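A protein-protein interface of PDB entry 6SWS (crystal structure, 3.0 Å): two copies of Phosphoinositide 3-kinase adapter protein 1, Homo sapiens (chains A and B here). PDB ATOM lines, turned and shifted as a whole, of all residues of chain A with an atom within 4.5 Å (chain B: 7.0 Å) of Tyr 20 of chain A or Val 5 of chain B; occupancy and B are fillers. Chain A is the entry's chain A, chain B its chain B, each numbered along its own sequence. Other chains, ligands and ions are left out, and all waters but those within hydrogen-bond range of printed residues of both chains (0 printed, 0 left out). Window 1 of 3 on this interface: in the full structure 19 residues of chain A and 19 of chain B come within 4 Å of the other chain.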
ATOM      1  N   VAL A   5      11.367  -0.179  21.770  1.00  0.00           N
ATOM      2  CA  VAL A   5      10.372   0.708  21.183  1.00  0.00           C
ATOM      3  C   VAL A   5       9.842   0.078  19.903  1.00  0.00           C
ATOM      4  O   VAL A   5      10.559  -0.626  19.185  1.00  0.00           O
ATOM      5  CB  VAL A   5      10.934   2.126  20.896  1.00  0.00           C
ATOM      6  CG1 VAL A   5      11.745   2.644  22.076  1.00  0.00           C
ATOM      7  CG2 VAL A   5      11.764   2.136  19.630  1.00  0.00           C
ATOM      8  N   VAL A   6       8.560   0.312  19.641  1.00  0.00           N
ATOM      9  CA  VAL A   6       7.905  -0.114  18.410  1.00  0.00           C
ATOM     10  C   VAL A   6       7.215   1.129  17.867  1.00  0.00           C
ATOM     11  O   VAL A   6       6.150   1.519  18.356  1.00  0.00           O
ATOM     12  CB  VAL A   6       6.905  -1.252  18.638  1.00  0.00           C
ATOM     13  CG1 VAL A   6       6.256  -1.657  17.325  1.00  0.00           C
ATOM     14  CG2 VAL A   6       7.597  -2.436  19.288  1.00  0.00           C
ATOM     15  N   GLN A   7       7.816   1.761  16.860  1.00  0.00           N
ATOM     16  CA  GLN A   7       7.328   3.041  16.386  1.00  0.00           C
ATOM     17  C   GLN A   7       7.205   3.015  14.867  1.00  0.00           C
ATOM     18  O   GLN A   7       8.166   2.636  14.173  1.00  0.00           O
ATOM     19  CB  GLN A   7       8.259   4.176  16.833  1.00  0.00           C
ATOM     20  CG  GLN A   7       7.542   5.482  17.130  1.00  0.00           C
ATOM     21  CD  GLN A   7       6.750   5.430  18.424  1.00  0.00           C
ATOM     22  OE1 GLN A   7       6.935   4.528  19.241  1.00  0.00           O
ATOM     23  NE2 GLN A   7       5.854   6.392  18.610  1.00  0.00           N
ATOM     24  N   THR A  18       5.603   2.035   7.499  1.00  0.00           N
ATOM     25  CA  THR A  18       6.702   1.167   7.897  1.00  0.00           C
ATOM     26  C   THR A  18       6.865   1.222   9.409  1.00  0.00           C
ATOM     27  O   THR A  18       6.968   2.308   9.989  1.00  0.00           O
ATOM     28  CB  THR A  18       8.001   1.587   7.208  1.00  0.00           C
ATOM     29  OG1 THR A  18       7.838   1.482   5.788  1.00  0.00           O
ATOM     30  CG2 THR A  18       9.150   0.695   7.651  1.00  0.00           C
ATOM     31  N   VAL A  19       6.888   0.055  10.042  1.00  0.00           N
ATOM     32  CA  VAL A  19       7.044  -0.072  11.485  1.00  0.00           C
ATOM     33  C   VAL A  19       8.489  -0.448  11.784  1.00  0.00           C
ATOM     34  O   VAL A  19       9.066  -1.316  11.112  1.00  0.00           O
ATOM     35  CB  VAL A  19       6.065  -1.112  12.055  1.00  0.00           C
ATOM     36  CG1 VAL A  19       6.254  -1.269  13.556  1.00  0.00           C
ATOM     37  CG2 VAL A  19       4.634  -0.712  11.735  1.00  0.00           C
ATOM     38  N   TYR A  20       9.080   0.219  12.774  1.00  0.00           N
ATOM     39  CA  TYR A  20      10.443  -0.042  13.213  1.00  0.00           C
ATOM     40  C   TYR A  20      10.417  -0.577  14.638  1.00  0.00           C
ATOM     41  O   TYR A  20       9.756  -0.002  15.508  1.00  0.00           O
ATOM     42  CB  TYR A  20      11.293   1.229  13.147  1.00  0.00           C
ATOM     43  CG  TYR A  20      11.406   1.807  11.758  1.00  0.00           C
ATOM     44  CD1 TYR A  20      12.394   1.380  10.886  1.00  0.00           C
ATOM     45  CD2 TYR A  20      10.531   2.792  11.324  1.00  0.00           C
ATOM     46  CE1 TYR A  20      12.496   1.906   9.617  1.00  0.00           C
ATOM     47  CE2 TYR A  20      10.630   3.326  10.056  1.00  0.00           C
ATOM     48  CZ  TYR A  20      11.618   2.881   9.206  1.00  0.00           C
ATOM     49  OH  TYR A  20      11.727   3.408   7.939  1.00  0.00           O
ATOM     50  N   VAL A  21      11.128  -1.676  14.869  1.00  0.00           N
ATOM     51  CA  VAL A  21      11.217  -2.309  16.181  1.00  0.00           C
ATOM     52  C   VAL A  21      12.677  -2.309  16.615  1.00  0.00           C
ATOM     53  O   VAL A  21      13.536  -2.861  15.917  1.00  0.00           O
ATOM     54  CB  VAL A  21      10.654  -3.738  16.170  1.00  0.00           C
ATOM     55  CG1 VAL A  21      10.900  -4.407  17.512  1.00  0.00           C
ATOM     56  CG2 VAL A  21       9.170  -3.725  15.839  1.00  0.00           C
ATOM     57  N   ILE A  22      12.953  -1.687  17.756  1.00  0.00           N
ATOM     58  CA  ILE A  22      14.282  -1.701  18.358  1.00  0.00           C
ATOM     59  C   ILE A  22      14.337  -2.838  19.371  1.00  0.00           C
ATOM     60  O   ILE A  22      13.502  -2.909  20.278  1.00  0.00           O
ATOM     61  CB  ILE A  22      14.610  -0.356  19.023  1.00  0.00           C
ATOM     62  CG1 ILE A  22      14.587   0.776  17.992  1.00  0.00           C
ATOM     63  CG2 ILE A  22      15.965  -0.420  19.714  1.00  0.00           C
ATOM     64  CD1 ILE A  22      15.542   0.582  16.849  1.00  0.00           C
ATOM     65  N   ILE A  57      14.716  -3.702  13.382  1.00  0.00           N
ATOM     66  CA  ILE A  57      13.941  -4.415  12.370  1.00  0.00           C
ATOM     67  C   ILE A  57      12.955  -3.440  11.746  1.00  0.00           C
ATOM     68  O   ILE A  57      12.389  -2.591  12.443  1.00  0.00           O
ATOM     69  CB  ILE A  57      13.165  -5.605  12.968  1.00  0.00           C
ATOM     70  CG1 ILE A  57      14.070  -6.453  13.846  1.00  0.00           C
ATOM     71  CG2 ILE A  57      12.560  -6.466  11.863  1.00  0.00           C
ATOM     72  CD1 ILE A  57      13.321  -7.262  14.875  1.00  0.00           C
ATOM     73  N   SER A  58      12.736  -3.568  10.441  1.00  0.00           N
ATOM     74  CA  SER A  58      11.737  -2.778   9.735  1.00  0.00           C
ATOM     75  C   SER A  58      10.765  -3.708   9.025  1.00  0.00           C
ATOM     76  O   SER A  58      11.165  -4.754   8.504  1.00  0.00           O
ATOM     77  CB  SER A  58      12.383  -1.839   8.719  1.00  0.00           C
ATOM     78  OG  SER A  58      12.594  -2.507   7.489  1.00  0.00           O
ATOM     79  N   ASN B   2      23.367   9.480   6.403  1.00  0.00           N
ATOM     80  CA  ASN B   2      23.746   8.695   7.569  1.00  0.00           C
ATOM     81  C   ASN B   2      22.564   8.444   8.492  1.00  0.00           C
ATOM     82  O   ASN B   2      22.576   7.462   9.244  1.00  0.00           O
ATOM     83  CB  ASN B   2      24.868   9.404   8.330  1.00  0.00           C
ATOM     84  CG  ASN B   2      25.412   8.575   9.475  1.00  0.00           C
ATOM     85  OD1 ASN B   2      25.534   7.355   9.370  1.00  0.00           O
ATOM     86  ND2 ASN B   2      25.749   9.238  10.576  1.00  0.00           N
ATOM     87  N   ALA B   3      21.552   9.307   8.455  1.00  0.00           N
ATOM     88  CA  ALA B   3      20.332   9.107   9.229  1.00  0.00           C
ATOM     89  C   ALA B   3      19.401   8.206   8.429  1.00  0.00           C
ATOM     90  O   ALA B   3      18.811   8.637   7.432  1.00  0.00           O
ATOM     91  CB  ALA B   3      19.671  10.443   9.552  1.00  0.00           C
ATOM     92  N   MET B   4      19.268   6.954   8.861  1.00  0.00           N
ATOM     93  CA  MET B   4      18.422   6.009   8.144  1.00  0.00           C
ATOM     94  C   MET B   4      16.953   6.410   8.220  1.00  0.00           C
ATOM     95  O   MET B   4      16.253   6.436   7.200  1.00  0.00           O
ATOM     96  CB  MET B   4      18.622   4.607   8.711  1.00  0.00           C
ATOM     97  CG  MET B   4      17.575   3.634   8.248  1.00  0.00           C
ATOM     98  SD  MET B   4      17.484   2.190   9.306  1.00  0.00           S
ATOM     99  CE  MET B   4      15.779   1.761   9.024  1.00  0.00           C
ATOM    100  N   VAL B   5      16.464   6.708   9.419  1.00  0.00           N
ATOM    101  CA  VAL B   5      15.067   7.082   9.617  1.00  0.00           C
ATOM    102  C   VAL B   5      14.983   7.982  10.839  1.00  0.00           C
ATOM    103  O   VAL B   5      15.669   7.755  11.841  1.00  0.00           O
ATOM    104  CB  VAL B   5      14.165   5.837   9.759  1.00  0.00           C
ATOM    105  CG1 VAL B   5      14.699   4.911  10.832  1.00  0.00           C
ATOM    106  CG2 VAL B   5      12.731   6.243  10.060  1.00  0.00           C
ATOM    107  N   VAL B   6      14.157   9.019  10.748  1.00  0.00           N
ATOM    108  CA  VAL B   6      13.834   9.856  11.895  1.00  0.00           C
ATOM    109  C   VAL B   6      12.350   9.664  12.191  1.00  0.00           C
ATOM    110  O   VAL B   6      11.485  10.306  11.584  1.00  0.00           O
ATOM    111  CB  VAL B   6      14.180  11.325  11.632  1.00  0.00           C
ATOM    112  CG1 VAL B   6      13.855  12.180  12.838  1.00  0.00           C
ATOM    113  CG2 VAL B   6      15.648  11.444  11.275  1.00  0.00           C
ATOM    114  N   GLN B   7      12.060   8.765  13.130  1.00  0.00           N
ATOM    115  CA  GLN B   7      10.701   8.356  13.448  1.00  0.00           C
ATOM    116  C   GLN B   7      10.255   9.061  14.722  1.00  0.00           C
ATOM    117  O   GLN B   7      10.834   8.801  15.789  1.00  0.00           O
ATOM    118  CB  GLN B   7      10.633   6.840  13.622  1.00  0.00           C
ATOM    119  CG  GLN B   7       9.301   6.295  14.102  1.00  0.00           C
ATOM    120  CD  GLN B   7       8.147   6.673  13.197  1.00  0.00           C
ATOM    121  OE1 GLN B   7       8.307   6.788  11.983  1.00  0.00           O
ATOM    122  NE2 GLN B   7       6.969   6.854  13.785  1.00  0.00           N
ATOM    123  N   PRO B   8       9.246   9.946  14.685  1.00  0.00           N
ATOM    124  CA  PRO B   8       8.496  10.466  13.539  1.00  0.00           C
ATOM    125  C   PRO B   8       9.099  11.732  12.938  1.00  0.00           C
ATOM    126  O   PRO B   8       9.761  12.496  13.640  1.00  0.00           O
ATOM    127  CB  PRO B   8       7.114  10.774  14.134  1.00  0.00           C
ATOM    128  CG  PRO B   8       7.277  10.685  15.644  1.00  0.00           C
ATOM    129  CD  PRO B   8       8.721  10.483  15.949  1.00  0.00           C
ATOM    130  N   TYR B  20      13.033   9.412  17.536  1.00  0.00           N
ATOM    131  CA  TYR B  20      14.066   8.394  17.430  1.00  0.00           C
ATOM    132  C   TYR B  20      14.794   8.565  16.107  1.00  0.00           C
ATOM    133  O   TYR B  20      14.159   8.731  15.060  1.00  0.00           O
ATOM    134  CB  TYR B  20      13.468   6.988  17.522  1.00  0.00           C
ATOM    135  CG  TYR B  20      12.876   6.667  18.873  1.00  0.00           C
ATOM    136  CD1 TYR B  20      13.659   6.134  19.887  1.00  0.00           C
ATOM    137  CD2 TYR B  20      11.536   6.909  19.139  1.00  0.00           C
ATOM    138  CE1 TYR B  20      13.124   5.847  21.126  1.00  0.00           C
ATOM    139  CE2 TYR B  20      10.991   6.625  20.375  1.00  0.00           C
ATOM    140  CZ  TYR B  20      11.789   6.095  21.364  1.00  0.00           C
ATOM    141  OH  TYR B  20      11.249   5.811  22.597  1.00  0.00           O
ATOM    142  N   VAL B  21      16.121   8.510  16.159  1.00  0.00           N
ATOM    143  CA  VAL B  21      16.968   8.634  14.981  1.00  0.00           C
ATOM    144  C   VAL B  21      17.863   7.409  14.931  1.00  0.00           C
ATOM    145  O   VAL B  21      18.693   7.207  15.827  1.00  0.00           O
ATOM    146  CB  VAL B  21      17.816   9.917  15.004  1.00  0.00           C
ATOM    147  CG1 VAL B  21      18.838   9.895  13.878  1.00  0.00           C
ATOM    148  CG2 VAL B  21      16.932  11.144  14.890  1.00  0.00           C
ATOM    149  N   ILE B  22      17.691   6.596  13.903  1.00  0.00           N
ATOM    150  CA  ILE B  22      18.555   5.449  13.663  1.00  0.00           C
ATOM    151  C   ILE B  22      19.667   5.884  12.723  1.00  0.00           C
ATOM    152  O   ILE B  22      19.423   6.572  11.724  1.00  0.00           O
ATOM    153  CB  ILE B  22      17.762   4.262  13.087  1.00  0.00           C
ATOM    154  CG1 ILE B  22      16.426   4.097  13.818  1.00  0.00           C
ATOM    155  CG2 ILE B  22      18.584   2.982  13.179  1.00  0.00           C
ATOM    156  CD1 ILE B  22      16.566   3.728  15.272  1.00  0.00           C
ATOM    157  N   VAL B  23      20.892   5.477  13.033  1.00  0.00           N
ATOM    158  CA  VAL B  23      22.061   5.892  12.273  1.00  0.00           C
ATOM    159  C   VAL B  23      22.687   4.655  11.646  1.00  0.00           C
ATOM    160  O   VAL B  23      22.552   3.539  12.158  1.00  0.00           O
ATOM    161  CB  VAL B  23      23.064   6.638  13.186  1.00  0.00           C
ATOM    162  CG1 VAL B  23      24.303   7.059  12.427  1.00  0.00           C
ATOM    163  CG2 VAL B  23      22.397   7.846  13.828  1.00  0.00           C
ATOM    164  N   ARG B  24      23.373   4.860  10.522  1.00  0.00           N
ATOM    165  CA  ARG B  24      24.055   3.777   9.827  1.00  0.00           C
ATOM    166  C   ARG B  24      25.447   3.522  10.389  1.00  0.00           C
ATOM    167  O   ARG B  24      25.866   2.366  10.502  1.00  0.00           O
ATOM    168  CB  ARG B  24      24.134   4.092   8.331  1.00  0.00           C
ATOM    169  CG  ARG B  24      22.809   3.904   7.611  1.00  0.00           C
ATOM    170  CD  ARG B  24      22.919   4.168   6.119  1.00  0.00           C
ATOM    171  NE  ARG B  24      21.810   3.563   5.388  1.00  0.00           N
ATOM    172  CZ  ARG B  24      20.690   4.205   5.073  1.00  0.00           C
ATOM    173  NH1 ARG B  24      20.525   5.472   5.428  1.00  0.00           N
ATOM    174  NH2 ARG B  24      19.730   3.577   4.409  1.00  0.00           N
ATOM    175  N   CYS B  81      23.430  13.401  12.043  1.00  0.00           N
ATOM    176  CA  CYS B  81      22.108  13.461  11.435  1.00  0.00           C
ATOM    177  C   CYS B  81      21.747  14.915  11.181  1.00  0.00           C
ATOM    178  O   CYS B  81      21.882  15.754  12.076  1.00  0.00           O
ATOM    179  CB  CYS B  81      21.055  12.803  12.332  1.00  0.00           C
ATOM    180  SG  CYS B  81      19.350  13.179  11.867  1.00  0.00           S
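The backbone carbonyl oxygen (O) of Val 5 of chain A is in hydrogen-bond range of the backbone NH (N) of Ile 22 of chain A, 3.0 Å away. The backbone NH (N) of Tyr 20 of chain A is in hydrogen-bond range of the backbone carbonyl oxygen (O) of Gln 7 of chain A (2.9 Å). N of Met 4 of chain B sits at hydrogen-bond distance from O of Ile 22 of chain B, 2.9 Å away. N of Ile 22 of chain B lies within hydrogen-bond range of O of Val 5 of chain B (3.1 Å). The backbone NH (N) of Gln 7 of chain B lies within hydrogen-bond range of the backbone carbonyl oxygen (O) of Tyr 20 of chain B, at 2.9 Å.
Val 5 of chain A touches Tyr 20 of chain B. Gln 7 of chain A touches Gln 7 of chain B (CG to CG, 3.6 Å). Met 4 of chain B touches Tyr 20 of chain A (CE to CE1, 3.3 Å). Tyr 20 of chain A touches Val 5 of chain B (CE2 to CG2, 3.6 Å). Ile 22 of chain B touches Ile 22 of chain A.
Of chain B, only Met 4 and Val 5 come within 4 Å of Tyr 20 of chain A. Of the printed residues of chain A, Gln 7 of chain B touches Gln 7. Of the printed residues of chain A, Ile 22 of chain B touches Ile 22. Ser 58 of chain A touches none of the printed residues of chain B. The nearest printed residue of chain A that does not touch Gln 7 of chain B is Tyr 20 of chain A (4.6 Å).
Printed residues of chain B that touch a printed residue of chain A: Met 4, Val 5, Gln 7, Tyr 20 and Ile 22. Of the 10 printed residues of chain A, 4 touch a printed residue of chain B. Hydrophobic or aromatic side chains of chain A that line the printed part of chain B: Val 5, Tyr 20 and Ile 22. Among the printed residues, no Asp or Glu carboxylate lies within 4 Å of a Lys or Arg side-chain nitrogen of the other chain.
Val 5 of chain A touches Tyr 20 of chain B, and with the chains exchanged Tyr 20 of chain A touches Val 5 of chain B. Gln 7 of chain A touches its own counterpart, Gln 7 of chain B. Ile 22 of chain B touches its own counterpart, Ile 22 of chain A. Positions printed for both chains: 5, 6, 7, 20, 21 and 22. Of the 5 pairs that touch across the chains among the printed residues, 4 have their exchanged pair printed and touching as well.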
